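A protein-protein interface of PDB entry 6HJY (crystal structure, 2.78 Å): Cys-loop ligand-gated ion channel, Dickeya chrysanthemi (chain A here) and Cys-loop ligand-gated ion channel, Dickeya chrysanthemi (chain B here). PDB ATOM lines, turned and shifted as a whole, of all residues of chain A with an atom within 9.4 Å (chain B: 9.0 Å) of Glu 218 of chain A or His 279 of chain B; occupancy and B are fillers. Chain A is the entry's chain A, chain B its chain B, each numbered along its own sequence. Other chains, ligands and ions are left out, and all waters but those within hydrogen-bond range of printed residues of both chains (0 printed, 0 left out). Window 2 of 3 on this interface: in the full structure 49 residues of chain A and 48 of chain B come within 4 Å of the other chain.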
ATOM      1  N   SER A 213     -33.941 -31.648 -23.700  1.00  0.00           N
ATOM      2  CA  SER A 213     -32.588 -31.156 -23.995  1.00  0.00           C
ATOM      3  C   SER A 213     -32.236 -29.877 -23.207  1.00  0.00           C
ATOM      4  O   SER A 213     -31.082 -29.441 -23.231  1.00  0.00           O
ATOM      5  CB  SER A 213     -32.406 -30.944 -25.498  1.00  0.00           C
ATOM      6  OG  SER A 213     -32.961 -29.721 -25.954  1.00  0.00           O
ATOM      7  N   VAL A 214     -33.227 -29.300 -22.495  1.00  0.00           N
ATOM      8  CA  VAL A 214     -33.091 -28.092 -21.672  1.00  0.00           C
ATOM      9  C   VAL A 214     -32.183 -28.327 -20.452  1.00  0.00           C
ATOM     10  O   VAL A 214     -31.532 -27.390 -19.998  1.00  0.00           O
ATOM     11  CB  VAL A 214     -34.454 -27.443 -21.276  1.00  0.00           C
ATOM     12  CG1 VAL A 214     -35.262 -27.038 -22.509  1.00  0.00           C
ATOM     13  CG2 VAL A 214     -35.278 -28.328 -20.341  1.00  0.00           C
ATOM     14  N   PHE A 215     -32.135 -29.582 -19.947  1.00  0.00           N
ATOM     15  CA  PHE A 215     -31.342 -30.010 -18.792  1.00  0.00           C
ATOM     16  C   PHE A 215     -29.838 -29.961 -19.058  1.00  0.00           C
ATOM     17  O   PHE A 215     -29.045 -29.934 -18.111  1.00  0.00           O
ATOM     18  CB  PHE A 215     -31.779 -31.410 -18.333  1.00  0.00           C
ATOM     19  CG  PHE A 215     -33.131 -31.435 -17.664  1.00  0.00           C
ATOM     20  CD1 PHE A 215     -33.246 -31.305 -16.285  1.00  0.00           C
ATOM     21  CD2 PHE A 215     -34.291 -31.577 -18.413  1.00  0.00           C
ATOM     22  CE1 PHE A 215     -34.499 -31.316 -15.666  1.00  0.00           C
ATOM     23  CE2 PHE A 215     -35.543 -31.584 -17.795  1.00  0.00           C
ATOM     24  CZ  PHE A 215     -35.639 -31.454 -16.426  1.00  0.00           C
ATOM     25  N   TRP A 216     -29.453 -29.914 -20.347  1.00  0.00           N
ATOM     26  CA  TRP A 216     -28.066 -29.834 -20.800  1.00  0.00           C
ATOM     27  C   TRP A 216     -27.528 -28.392 -20.776  1.00  0.00           C
ATOM     28  O   TRP A 216     -26.346 -28.180 -21.059  1.00  0.00           O
ATOM     29  CB  TRP A 216     -27.899 -30.509 -22.171  1.00  0.00           C
ATOM     30  CG  TRP A 216     -28.233 -31.975 -22.143  1.00  0.00           C
ATOM     31  CD1 TRP A 216     -29.430 -32.550 -22.453  1.00  0.00           C
ATOM     32  CD2 TRP A 216     -27.365 -33.045 -21.736  1.00  0.00           C
ATOM     33  NE1 TRP A 216     -29.360 -33.914 -22.286  1.00  0.00           N
ATOM     34  CE2 TRP A 216     -28.103 -34.247 -21.847  1.00  0.00           C
ATOM     35  CE3 TRP A 216     -26.034 -33.106 -21.290  1.00  0.00           C
ATOM     36  CZ2 TRP A 216     -27.548 -35.497 -21.537  1.00  0.00           C
ATOM     37  CZ3 TRP A 216     -25.481 -34.344 -20.992  1.00  0.00           C
ATOM     38  CH2 TRP A 216     -26.234 -35.522 -21.111  1.00  0.00           C
ATOM     39  N   LEU A 217     -28.386 -27.411 -20.401  1.00  0.00           N
ATOM     40  CA  LEU A 217     -28.010 -26.002 -20.253  1.00  0.00           C
ATOM     41  C   LEU A 217     -27.258 -25.830 -18.934  1.00  0.00           C
ATOM     42  O   LEU A 217     -27.593 -26.481 -17.937  1.00  0.00           O
ATOM     43  CB  LEU A 217     -29.236 -25.080 -20.305  1.00  0.00           C
ATOM     44  CG  LEU A 217     -29.771 -24.748 -21.690  1.00  0.00           C
ATOM     45  CD1 LEU A 217     -31.261 -24.461 -21.641  1.00  0.00           C
ATOM     46  CD2 LEU A 217     -29.018 -23.568 -22.305  1.00  0.00           C
ATOM     47  N   GLU A 218     -26.248 -24.947 -18.935  1.00  0.00           N
ATOM     48  CA  GLU A 218     -25.344 -24.708 -17.812  1.00  0.00           C
ATOM     49  C   GLU A 218     -26.006 -24.079 -16.576  1.00  0.00           C
ATOM     50  O   GLU A 218     -25.961 -24.689 -15.504  1.00  0.00           O
ATOM     51  CB  GLU A 218     -24.106 -23.890 -18.252  1.00  0.00           C
ATOM     52  CG  GLU A 218     -23.317 -24.481 -19.417  1.00  0.00           C
ATOM     53  CD  GLU A 218     -22.795 -25.892 -19.209  1.00  0.00           C
ATOM     54  OE1 GLU A 218     -21.786 -26.053 -18.485  1.00  0.00           O
ATOM     55  OE2 GLU A 218     -23.411 -26.840 -19.748  1.00  0.00           O
ATOM     56  N   SER A 219     -26.597 -22.875 -16.710  1.00  0.00           N
ATOM     57  CA  SER A 219     -27.212 -22.163 -15.585  1.00  0.00           C
ATOM     58  C   SER A 219     -28.721 -22.367 -15.447  1.00  0.00           C
ATOM     59  O   SER A 219     -29.386 -22.795 -16.391  1.00  0.00           O
ATOM     60  CB  SER A 219     -26.869 -20.674 -15.637  1.00  0.00           C
ATOM     61  OG  SER A 219     -27.624 -19.984 -16.618  1.00  0.00           O
ATOM     62  N   PHE A 220     -29.246 -22.053 -14.242  1.00  0.00           N
ATOM     63  CA  PHE A 220     -30.660 -22.122 -13.862  1.00  0.00           C
ATOM     64  C   PHE A 220     -31.476 -21.099 -14.659  1.00  0.00           C
ATOM     65  O   PHE A 220     -32.622 -21.382 -15.025  1.00  0.00           O
ATOM     66  CB  PHE A 220     -30.799 -21.875 -12.344  1.00  0.00           C
ATOM     67  CG  PHE A 220     -32.202 -21.672 -11.811  1.00  0.00           C
ATOM     68  CD1 PHE A 220     -33.077 -22.743 -11.688  1.00  0.00           C
ATOM     69  CD2 PHE A 220     -32.630 -20.419 -11.387  1.00  0.00           C
ATOM     70  CE1 PHE A 220     -34.368 -22.561 -11.177  1.00  0.00           C
ATOM     71  CE2 PHE A 220     -33.922 -20.236 -10.876  1.00  0.00           C
ATOM     72  CZ  PHE A 220     -34.780 -21.309 -10.776  1.00  0.00           C
ATOM     73  N   SER A 221     -30.872 -19.920 -14.934  1.00  0.00           N
ATOM     74  CA  SER A 221     -31.449 -18.811 -15.705  1.00  0.00           C
ATOM     75  C   SER A 221     -31.721 -19.229 -17.153  1.00  0.00           C
ATOM     76  O   SER A 221     -32.745 -18.840 -17.720  1.00  0.00           O
ATOM     77  CB  SER A 221     -30.523 -17.602 -15.674  1.00  0.00           C
ATOM     78  OG  SER A 221     -31.102 -16.475 -16.312  1.00  0.00           O
ATOM     79  N   GLU A 222     -30.809 -20.037 -17.735  1.00  0.00           N
ATOM     80  CA  GLU A 222     -30.905 -20.558 -19.101  1.00  0.00           C
ATOM     81  C   GLU A 222     -31.953 -21.673 -19.190  1.00  0.00           C
ATOM     82  O   GLU A 222     -32.782 -21.640 -20.100  1.00  0.00           O
ATOM     83  CB  GLU A 222     -29.535 -21.071 -19.588  1.00  0.00           C
ATOM     84  CG  GLU A 222     -28.533 -19.970 -19.895  1.00  0.00           C
ATOM     85  CD  GLU A 222     -27.081 -20.419 -19.920  1.00  0.00           C
ATOM     86  OE1 GLU A 222     -26.763 -21.392 -20.643  1.00  0.00           O
ATOM     87  OE2 GLU A 222     -26.248 -19.770 -19.248  1.00  0.00           O
ATOM     88  N   ARG A 223     -31.916 -22.645 -18.239  1.00  0.00           N
ATOM     89  CA  ARG A 223     -32.817 -23.808 -18.154  1.00  0.00           C
ATOM     90  C   ARG A 223     -34.289 -23.418 -18.042  1.00  0.00           C
ATOM     91  O   ARG A 223     -35.136 -24.046 -18.679  1.00  0.00           O
ATOM     92  CB  ARG A 223     -32.441 -24.721 -16.973  1.00  0.00           C
ATOM     93  CG  ARG A 223     -31.199 -25.563 -17.215  1.00  0.00           C
ATOM     94  CD  ARG A 223     -31.037 -26.661 -16.179  1.00  0.00           C
ATOM     95  NE  ARG A 223     -30.780 -26.132 -14.838  1.00  0.00           N
ATOM     96  CZ  ARG A 223     -29.576 -25.837 -14.351  1.00  0.00           C
ATOM     97  NH1 ARG A 223     -28.492 -25.989 -15.104  1.00  0.00           N
ATOM     98  NH2 ARG A 223     -29.448 -25.377 -13.114  1.00  0.00           N
ATOM     99  N   LEU A 224     -34.591 -22.396 -17.219  1.00  0.00           N
ATOM    100  CA  LEU A 224     -35.953 -21.924 -16.985  1.00  0.00           C
ATOM    101  C   LEU A 224     -36.529 -21.144 -18.169  1.00  0.00           C
ATOM    102  O   LEU A 224     -37.610 -21.497 -18.641  1.00  0.00           O
ATOM    103  CB  LEU A 224     -36.036 -21.118 -15.675  1.00  0.00           C
ATOM    104  CG  LEU A 224     -37.433 -20.654 -15.222  1.00  0.00           C
ATOM    105  CD1 LEU A 224     -38.362 -21.834 -14.948  1.00  0.00           C
ATOM    106  CD2 LEU A 224     -37.337 -19.839 -13.977  1.00  0.00           C
ATOM    107  N   THR A 226     -35.787 -21.143 -21.252  1.00  0.00           N
ATOM    108  CA  THR A 226     -35.937 -22.013 -22.419  1.00  0.00           C
ATOM    109  C   THR A 226     -37.163 -22.929 -22.257  1.00  0.00           C
ATOM    110  O   THR A 226     -37.797 -23.279 -23.257  1.00  0.00           O
ATOM    111  CB  THR A 226     -34.624 -22.759 -22.709  1.00  0.00           C
ATOM    112  OG1 THR A 226     -33.542 -21.827 -22.695  1.00  0.00           O
ATOM    113  CG2 THR A 226     -34.639 -23.464 -24.047  1.00  0.00           C
ATOM    114  N   ILE A 272     -36.366 -28.715 -12.566  1.00  0.00           N
ATOM    115  CA  ILE A 272     -35.409 -27.598 -12.556  1.00  0.00           C
ATOM    116  C   ILE A 272     -35.435 -26.906 -11.180  1.00  0.00           C
ATOM    117  O   ILE A 272     -34.373 -26.683 -10.599  1.00  0.00           O
ATOM    118  CB  ILE A 272     -35.640 -26.615 -13.751  1.00  0.00           C
ATOM    119  CG1 ILE A 272     -35.360 -27.302 -15.103  1.00  0.00           C
ATOM    120  CG2 ILE A 272     -34.789 -25.335 -13.619  1.00  0.00           C
ATOM    121  CD1 ILE A 272     -36.100 -26.697 -16.306  1.00  0.00           C
ATOM    122  N   HIS A 276     -32.268 -26.089  -7.722  1.00  0.00           N
ATOM    123  CA  HIS A 276     -31.791 -24.775  -7.304  1.00  0.00           C
ATOM    124  C   HIS A 276     -32.215 -24.427  -5.874  1.00  0.00           C
ATOM    125  O   HIS A 276     -31.364 -24.422  -4.984  1.00  0.00           O
ATOM    126  CB  HIS A 276     -32.248 -23.700  -8.305  1.00  0.00           C
ATOM    127  CG  HIS A 276     -31.277 -22.571  -8.469  1.00  0.00           C
ATOM    128  ND1 HIS A 276     -31.631 -21.266  -8.181  1.00  0.00           N
ATOM    129  CD2 HIS A 276     -29.997 -22.591  -8.907  1.00  0.00           C
ATOM    130  CE1 HIS A 276     -30.562 -20.538  -8.450  1.00  0.00           C
ATOM    131  NE2 HIS A 276     -29.553 -21.291  -8.889  1.00  0.00           N
ATOM    132  N   GLU B 221     -21.190 -17.261 -31.082  1.00  0.00           N
ATOM    133  CA  GLU B 221     -20.023 -17.478 -30.228  1.00  0.00           C
ATOM    134  C   GLU B 221     -20.202 -18.551 -29.142  1.00  0.00           C
ATOM    135  O   GLU B 221     -19.426 -19.509 -29.124  1.00  0.00           O
ATOM    136  CB  GLU B 221     -19.530 -16.148 -29.609  1.00  0.00           C
ATOM    137  CG  GLU B 221     -19.273 -15.020 -30.603  1.00  0.00           C
ATOM    138  CD  GLU B 221     -18.308 -15.345 -31.728  1.00  0.00           C
ATOM    139  OE1 GLU B 221     -18.777 -15.554 -32.870  1.00  0.00           O
ATOM    140  OE2 GLU B 221     -17.088 -15.430 -31.461  1.00  0.00           O
ATOM    141  N   SER B 222     -21.188 -18.393 -28.239  1.00  0.00           N
ATOM    142  CA  SER B 222     -21.397 -19.335 -27.136  1.00  0.00           C
ATOM    143  C   SER B 222     -22.495 -20.376 -27.381  1.00  0.00           C
ATOM    144  O   SER B 222     -23.317 -20.217 -28.285  1.00  0.00           O
ATOM    145  CB  SER B 222     -21.642 -18.585 -25.826  1.00  0.00           C
ATOM    146  OG  SER B 222     -22.947 -18.033 -25.759  1.00  0.00           O
ATOM    147  N   PHE B 223     -22.484 -21.453 -26.562  1.00  0.00           N
ATOM    148  CA  PHE B 223     -23.446 -22.559 -26.577  1.00  0.00           C
ATOM    149  C   PHE B 223     -24.839 -22.065 -26.168  1.00  0.00           C
ATOM    150  O   PHE B 223     -25.841 -22.526 -26.726  1.00  0.00           O
ATOM    151  CB  PHE B 223     -22.966 -23.693 -25.643  1.00  0.00           C
ATOM    152  CG  PHE B 223     -23.953 -24.809 -25.366  1.00  0.00           C
ATOM    153  CD1 PHE B 223     -24.249 -25.757 -26.337  1.00  0.00           C
ATOM    154  CD2 PHE B 223     -24.555 -24.934 -24.118  1.00  0.00           C
ATOM    155  CE1 PHE B 223     -25.151 -26.796 -26.076  1.00  0.00           C
ATOM    156  CE2 PHE B 223     -25.457 -25.974 -23.857  1.00  0.00           C
ATOM    157  CZ  PHE B 223     -25.747 -26.897 -24.837  1.00  0.00           C
ATOM    158  N   SER B 224     -24.886 -21.116 -25.203  1.00  0.00           N
ATOM    159  CA  SER B 224     -26.101 -20.478 -24.675  1.00  0.00           C
ATOM    160  C   SER B 224     -26.830 -19.684 -25.767  1.00  0.00           C
ATOM    161  O   SER B 224     -28.062 -19.697 -25.810  1.00  0.00           O
ATOM    162  CB  SER B 224     -25.756 -19.568 -23.501  1.00  0.00           C
ATOM    163  OG  SER B 224     -26.916 -19.078 -22.848  1.00  0.00           O
ATOM    164  N   ARG B 226     -26.273 -20.152 -29.307  1.00  0.00           N
ATOM    165  CA  ARG B 226     -26.573 -21.123 -30.371  1.00  0.00           C
ATOM    166  C   ARG B 226     -27.898 -21.846 -30.135  1.00  0.00           C
ATOM    167  O   ARG B 226     -28.722 -21.925 -31.048  1.00  0.00           O
ATOM    168  CB  ARG B 226     -25.452 -22.171 -30.494  1.00  0.00           C
ATOM    169  CG  ARG B 226     -24.215 -21.688 -31.225  1.00  0.00           C
ATOM    170  CD  ARG B 226     -23.302 -22.848 -31.590  1.00  0.00           C
ATOM    171  NE  ARG B 226     -22.696 -23.482 -30.413  1.00  0.00           N
ATOM    172  CZ  ARG B 226     -21.554 -23.097 -29.846  1.00  0.00           C
ATOM    173  NH1 ARG B 226     -20.889 -22.050 -30.320  1.00  0.00           N
ATOM    174  NH2 ARG B 226     -21.075 -23.749 -28.796  1.00  0.00           N
ATOM    175  N   LEU B 227     -28.092 -22.367 -28.907  1.00  0.00           N
ATOM    176  CA  LEU B 227     -29.273 -23.121 -28.503  1.00  0.00           C
ATOM    177  C   LEU B 227     -30.549 -22.282 -28.453  1.00  0.00           C
ATOM    178  O   LEU B 227     -31.532 -22.663 -29.092  1.00  0.00           O
ATOM    179  CB  LEU B 227     -29.026 -23.847 -27.168  1.00  0.00           C
ATOM    180  CG  LEU B 227     -30.127 -24.806 -26.684  1.00  0.00           C
ATOM    181  CD1 LEU B 227     -30.350 -25.956 -27.667  1.00  0.00           C
ATOM    182  CD2 LEU B 227     -29.773 -25.377 -25.354  1.00  0.00           C
ATOM    183  N   ILE B 272     -29.772 -28.832 -33.922  1.00  0.00           N
ATOM    184  CA  ILE B 272     -29.831 -28.950 -32.461  1.00  0.00           C
ATOM    185  C   ILE B 272     -28.964 -30.130 -31.995  1.00  0.00           C
ATOM    186  O   ILE B 272     -28.190 -29.968 -31.049  1.00  0.00           O
ATOM    187  CB  ILE B 272     -31.306 -28.976 -31.934  1.00  0.00           C
ATOM    188  CG1 ILE B 272     -31.891 -27.549 -31.931  1.00  0.00           C
ATOM    189  CG2 ILE B 272     -31.430 -29.617 -30.524  1.00  0.00           C
ATOM    190  CD1 ILE B 272     -33.409 -27.419 -31.709  1.00  0.00           C
ATOM    191  N   LEU B 273     -29.046 -31.286 -32.697  1.00  0.00           N
ATOM    192  CA  LEU B 273     -28.236 -32.471 -32.396  1.00  0.00           C
ATOM    193  C   LEU B 273     -26.745 -32.185 -32.617  1.00  0.00           C
ATOM    194  O   LEU B 273     -25.913 -32.750 -31.908  1.00  0.00           O
ATOM    195  CB  LEU B 273     -28.674 -33.694 -33.229  1.00  0.00           C
ATOM    196  CG  LEU B 273     -29.979 -34.391 -32.830  1.00  0.00           C
ATOM    197  CD1 LEU B 273     -30.451 -35.309 -33.934  1.00  0.00           C
ATOM    198  CD2 LEU B 273     -29.831 -35.178 -31.520  1.00  0.00           C
ATOM    199  N   LEU B 274     -26.419 -31.293 -33.585  1.00  0.00           N
ATOM    200  CA  LEU B 274     -25.049 -30.886 -33.911  1.00  0.00           C
ATOM    201  C   LEU B 274     -24.449 -29.988 -32.821  1.00  0.00           C
ATOM    202  O   LEU B 274     -23.274 -30.159 -32.490  1.00  0.00           O
ATOM    203  CB  LEU B 274     -24.963 -30.195 -35.293  1.00  0.00           C
ATOM    204  CG  LEU B 274     -25.313 -31.033 -36.540  1.00  0.00           C
ATOM    205  CD1 LEU B 274     -25.449 -30.156 -37.763  1.00  0.00           C
ATOM    206  CD2 LEU B 274     -24.306 -32.159 -36.788  1.00  0.00           C
ATOM    207  N   ILE B 275     -25.255 -29.050 -32.258  1.00  0.00           N
ATOM    208  CA  ILE B 275     -24.853 -28.124 -31.185  1.00  0.00           C
ATOM    209  C   ILE B 275     -24.561 -28.905 -29.886  1.00  0.00           C
ATOM    210  O   ILE B 275     -23.567 -28.613 -29.218  1.00  0.00           O
ATOM    211  CB  ILE B 275     -25.879 -26.955 -30.995  1.00  0.00           C
ATOM    212  CG1 ILE B 275     -25.993 -26.093 -32.272  1.00  0.00           C
ATOM    213  CG2 ILE B 275     -25.526 -26.061 -29.784  1.00  0.00           C
ATOM    214  CD1 ILE B 275     -27.346 -25.365 -32.457  1.00  0.00           C
ATOM    215  N   ILE B 276     -25.406 -29.908 -29.555  1.00  0.00           N
ATOM    216  CA  ILE B 276     -25.248 -30.771 -28.374  1.00  0.00           C
ATOM    217  C   ILE B 276     -23.997 -31.659 -28.531  1.00  0.00           C
ATOM    218  O   ILE B 276     -23.249 -31.832 -27.565  1.00  0.00           O
ATOM    219  CB  ILE B 276     -26.546 -31.593 -28.068  1.00  0.00           C
ATOM    220  CG1 ILE B 276     -27.753 -30.666 -27.802  1.00  0.00           C
ATOM    221  CG2 ILE B 276     -26.347 -32.575 -26.887  1.00  0.00           C
ATOM    222  CD1 ILE B 276     -29.144 -31.311 -28.029  1.00  0.00           C
ATOM    223  N   PHE B 277     -23.737 -32.154 -29.761  1.00  0.00           N
ATOM    224  CA  PHE B 277     -22.590 -33.013 -30.082  1.00  0.00           C
ATOM    225  C   PHE B 277     -21.242 -32.247 -30.159  1.00  0.00           C
ATOM    226  O   PHE B 277     -20.283 -32.725 -30.772  1.00  0.00           O
ATOM    227  CB  PHE B 277     -22.862 -33.825 -31.365  1.00  0.00           C
ATOM    228  CG  PHE B 277     -22.363 -35.252 -31.312  1.00  0.00           C
ATOM    229  CD1 PHE B 277     -23.136 -36.257 -30.746  1.00  0.00           C
ATOM    230  CD2 PHE B 277     -21.121 -35.590 -31.833  1.00  0.00           C
ATOM    231  CE1 PHE B 277     -22.669 -37.574 -30.689  1.00  0.00           C
ATOM    232  CE2 PHE B 277     -20.653 -36.907 -31.774  1.00  0.00           C
ATOM    233  CZ  PHE B 277     -21.432 -37.889 -31.206  1.00  0.00           C
ATOM    234  N   ALA B 278     -21.167 -31.078 -29.509  1.00  0.00           N
ATOM    235  CA  ALA B 278     -19.960 -30.259 -29.445  1.00  0.00           C
ATOM    236  C   ALA B 278     -19.638 -29.889 -27.991  1.00  0.00           C
ATOM    237  O   ALA B 278     -18.483 -29.997 -27.579  1.00  0.00           O
ATOM    238  CB  ALA B 278     -20.141 -29.002 -30.284  1.00  0.00           C
ATOM    239  N   HIS B 279     -20.669 -29.489 -27.214  1.00  0.00           N
ATOM    240  CA  HIS B 279     -20.544 -29.083 -25.816  1.00  0.00           C
ATOM    241  C   HIS B 279     -20.289 -30.271 -24.884  1.00  0.00           C
ATOM    242  O   HIS B 279     -19.185 -30.379 -24.353  1.00  0.00           O
ATOM    243  CB  HIS B 279     -21.773 -28.262 -25.379  1.00  0.00           C
ATOM    244  CG  HIS B 279     -21.463 -27.190 -24.378  1.00  0.00           C
ATOM    245  ND1 HIS B 279     -22.092 -27.148 -23.147  1.00  0.00           N
ATOM    246  CD2 HIS B 279     -20.603 -26.149 -24.467  1.00  0.00           C
ATOM    247  CE1 HIS B 279     -21.600 -26.088 -22.530  1.00  0.00           C
ATOM    248  NE2 HIS B 279     -20.699 -25.456 -23.284  1.00  0.00           N
ATOM    249  N   HIS B 280     -21.283 -31.167 -24.701  1.00  0.00           N
ATOM    250  CA  HIS B 280     -21.151 -32.350 -23.843  1.00  0.00           C
ATOM    251  C   HIS B 280     -20.523 -33.527 -24.592  1.00  0.00           C
ATOM    252  O   HIS B 280     -20.787 -33.727 -25.777  1.00  0.00           O
ATOM    253  CB  HIS B 280     -22.511 -32.752 -23.250  1.00  0.00           C
ATOM    254  CG  HIS B 280     -22.963 -31.872 -22.123  1.00  0.00           C
ATOM    255  ND1 HIS B 280     -22.753 -32.223 -20.803  1.00  0.00           N
ATOM    256  CD2 HIS B 280     -23.624 -30.692 -22.160  1.00  0.00           C
ATOM    257  CE1 HIS B 280     -23.279 -31.248 -20.083  1.00  0.00           C
ATOM    258  NE2 HIS B 280     -23.818 -30.305 -20.853  1.00  0.00           N
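Of chain B, only His 279 (3.4 Å) and His 280 (3.7 Å) come within 4 Å of Glu 218 of chain A. No residue of chain B comes within 4 Å of Ser 219 of chain A. Ala 278 of chain B touches none of the printed residues of chain A. Of chain A, only Trp 216 (3.3 Å) and Glu 218 (3.7 Å) come within 4 Å of His 280 of chain B. Of the printed residues of chain A, Phe 223 of chain B touches Trp 216. Of the printed residues of chain A, Ser 224 of chain B touches Glu 222 (3.2 Å). Of the printed residues of chain B, Trp 216 of chain A touches Phe 223 (3.7 Å) and His 280 (3.3 Å). Printed residues of chain B within 4 Å of Leu 217 of chain A: Leu 227. Printed residues of chain B within 4 Å of Glu 222 of chain A: Ser 224. Leu 273 of chain B touches none of the printed residues of chain A. The nearest residue of chain A that does not touch His 279 of chain B is Trp 216 of chain A (4.8 Å). The nearest printed residue of chain B that does not touch Leu 217 of chain A is Phe 223 of chain B (4.4 Å).
O of Leu 217 of chain A is in hydrogen-bond range of NH1 of Arg 223 of chain A, 3.0 Å away. The backbone carbonyl oxygen of Glu 218 of chain A is in hydrogen-bond range of the guanidinium group of Arg 223 of chain A (2.9 Å). OG of Ser 219 of chain A sits at hydrogen-bond distance from OE2 of Glu 222 of chain A. The backbone carbonyl oxygen (O) of Glu 222 of chain A lies within hydrogen-bond range of the side-chain hydroxyl (OG1) of Thr 226 of chain A, 2.7 Å away.
Phe 223 of chain B touches Trp 216 of chain A (CE2 to O, 3.7 Å). Leu 217 of chain A touches Leu 227 of chain B. Glu 218 of chain A touches His 279 of chain B (OE2 to CE1, 3.4 Å). His 280 of chain B touches Glu 218 of chain A.
Printed residues of chain A that touch a printed residue of chain B: Trp 216, Leu 217, Glu 218 and Glu 222. Hydrophobic or aromatic side chains of chain A within 4 Å of the printed part of chain B: Trp 216 and Leu 217. Hydrophobic or aromatic side chains of chain B within 4 Å of the printed part of chain A: Phe 223, Leu 227, His 279 and His 280.
NE2 of His 280 of chain B lies within hydrogen-bond range of O of Trp 216 of chain A (3.3 Å). OE1 of Glu 222 of chain A is in hydrogen-bond range of OG of Ser 224 of chain B (3.2 Å).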
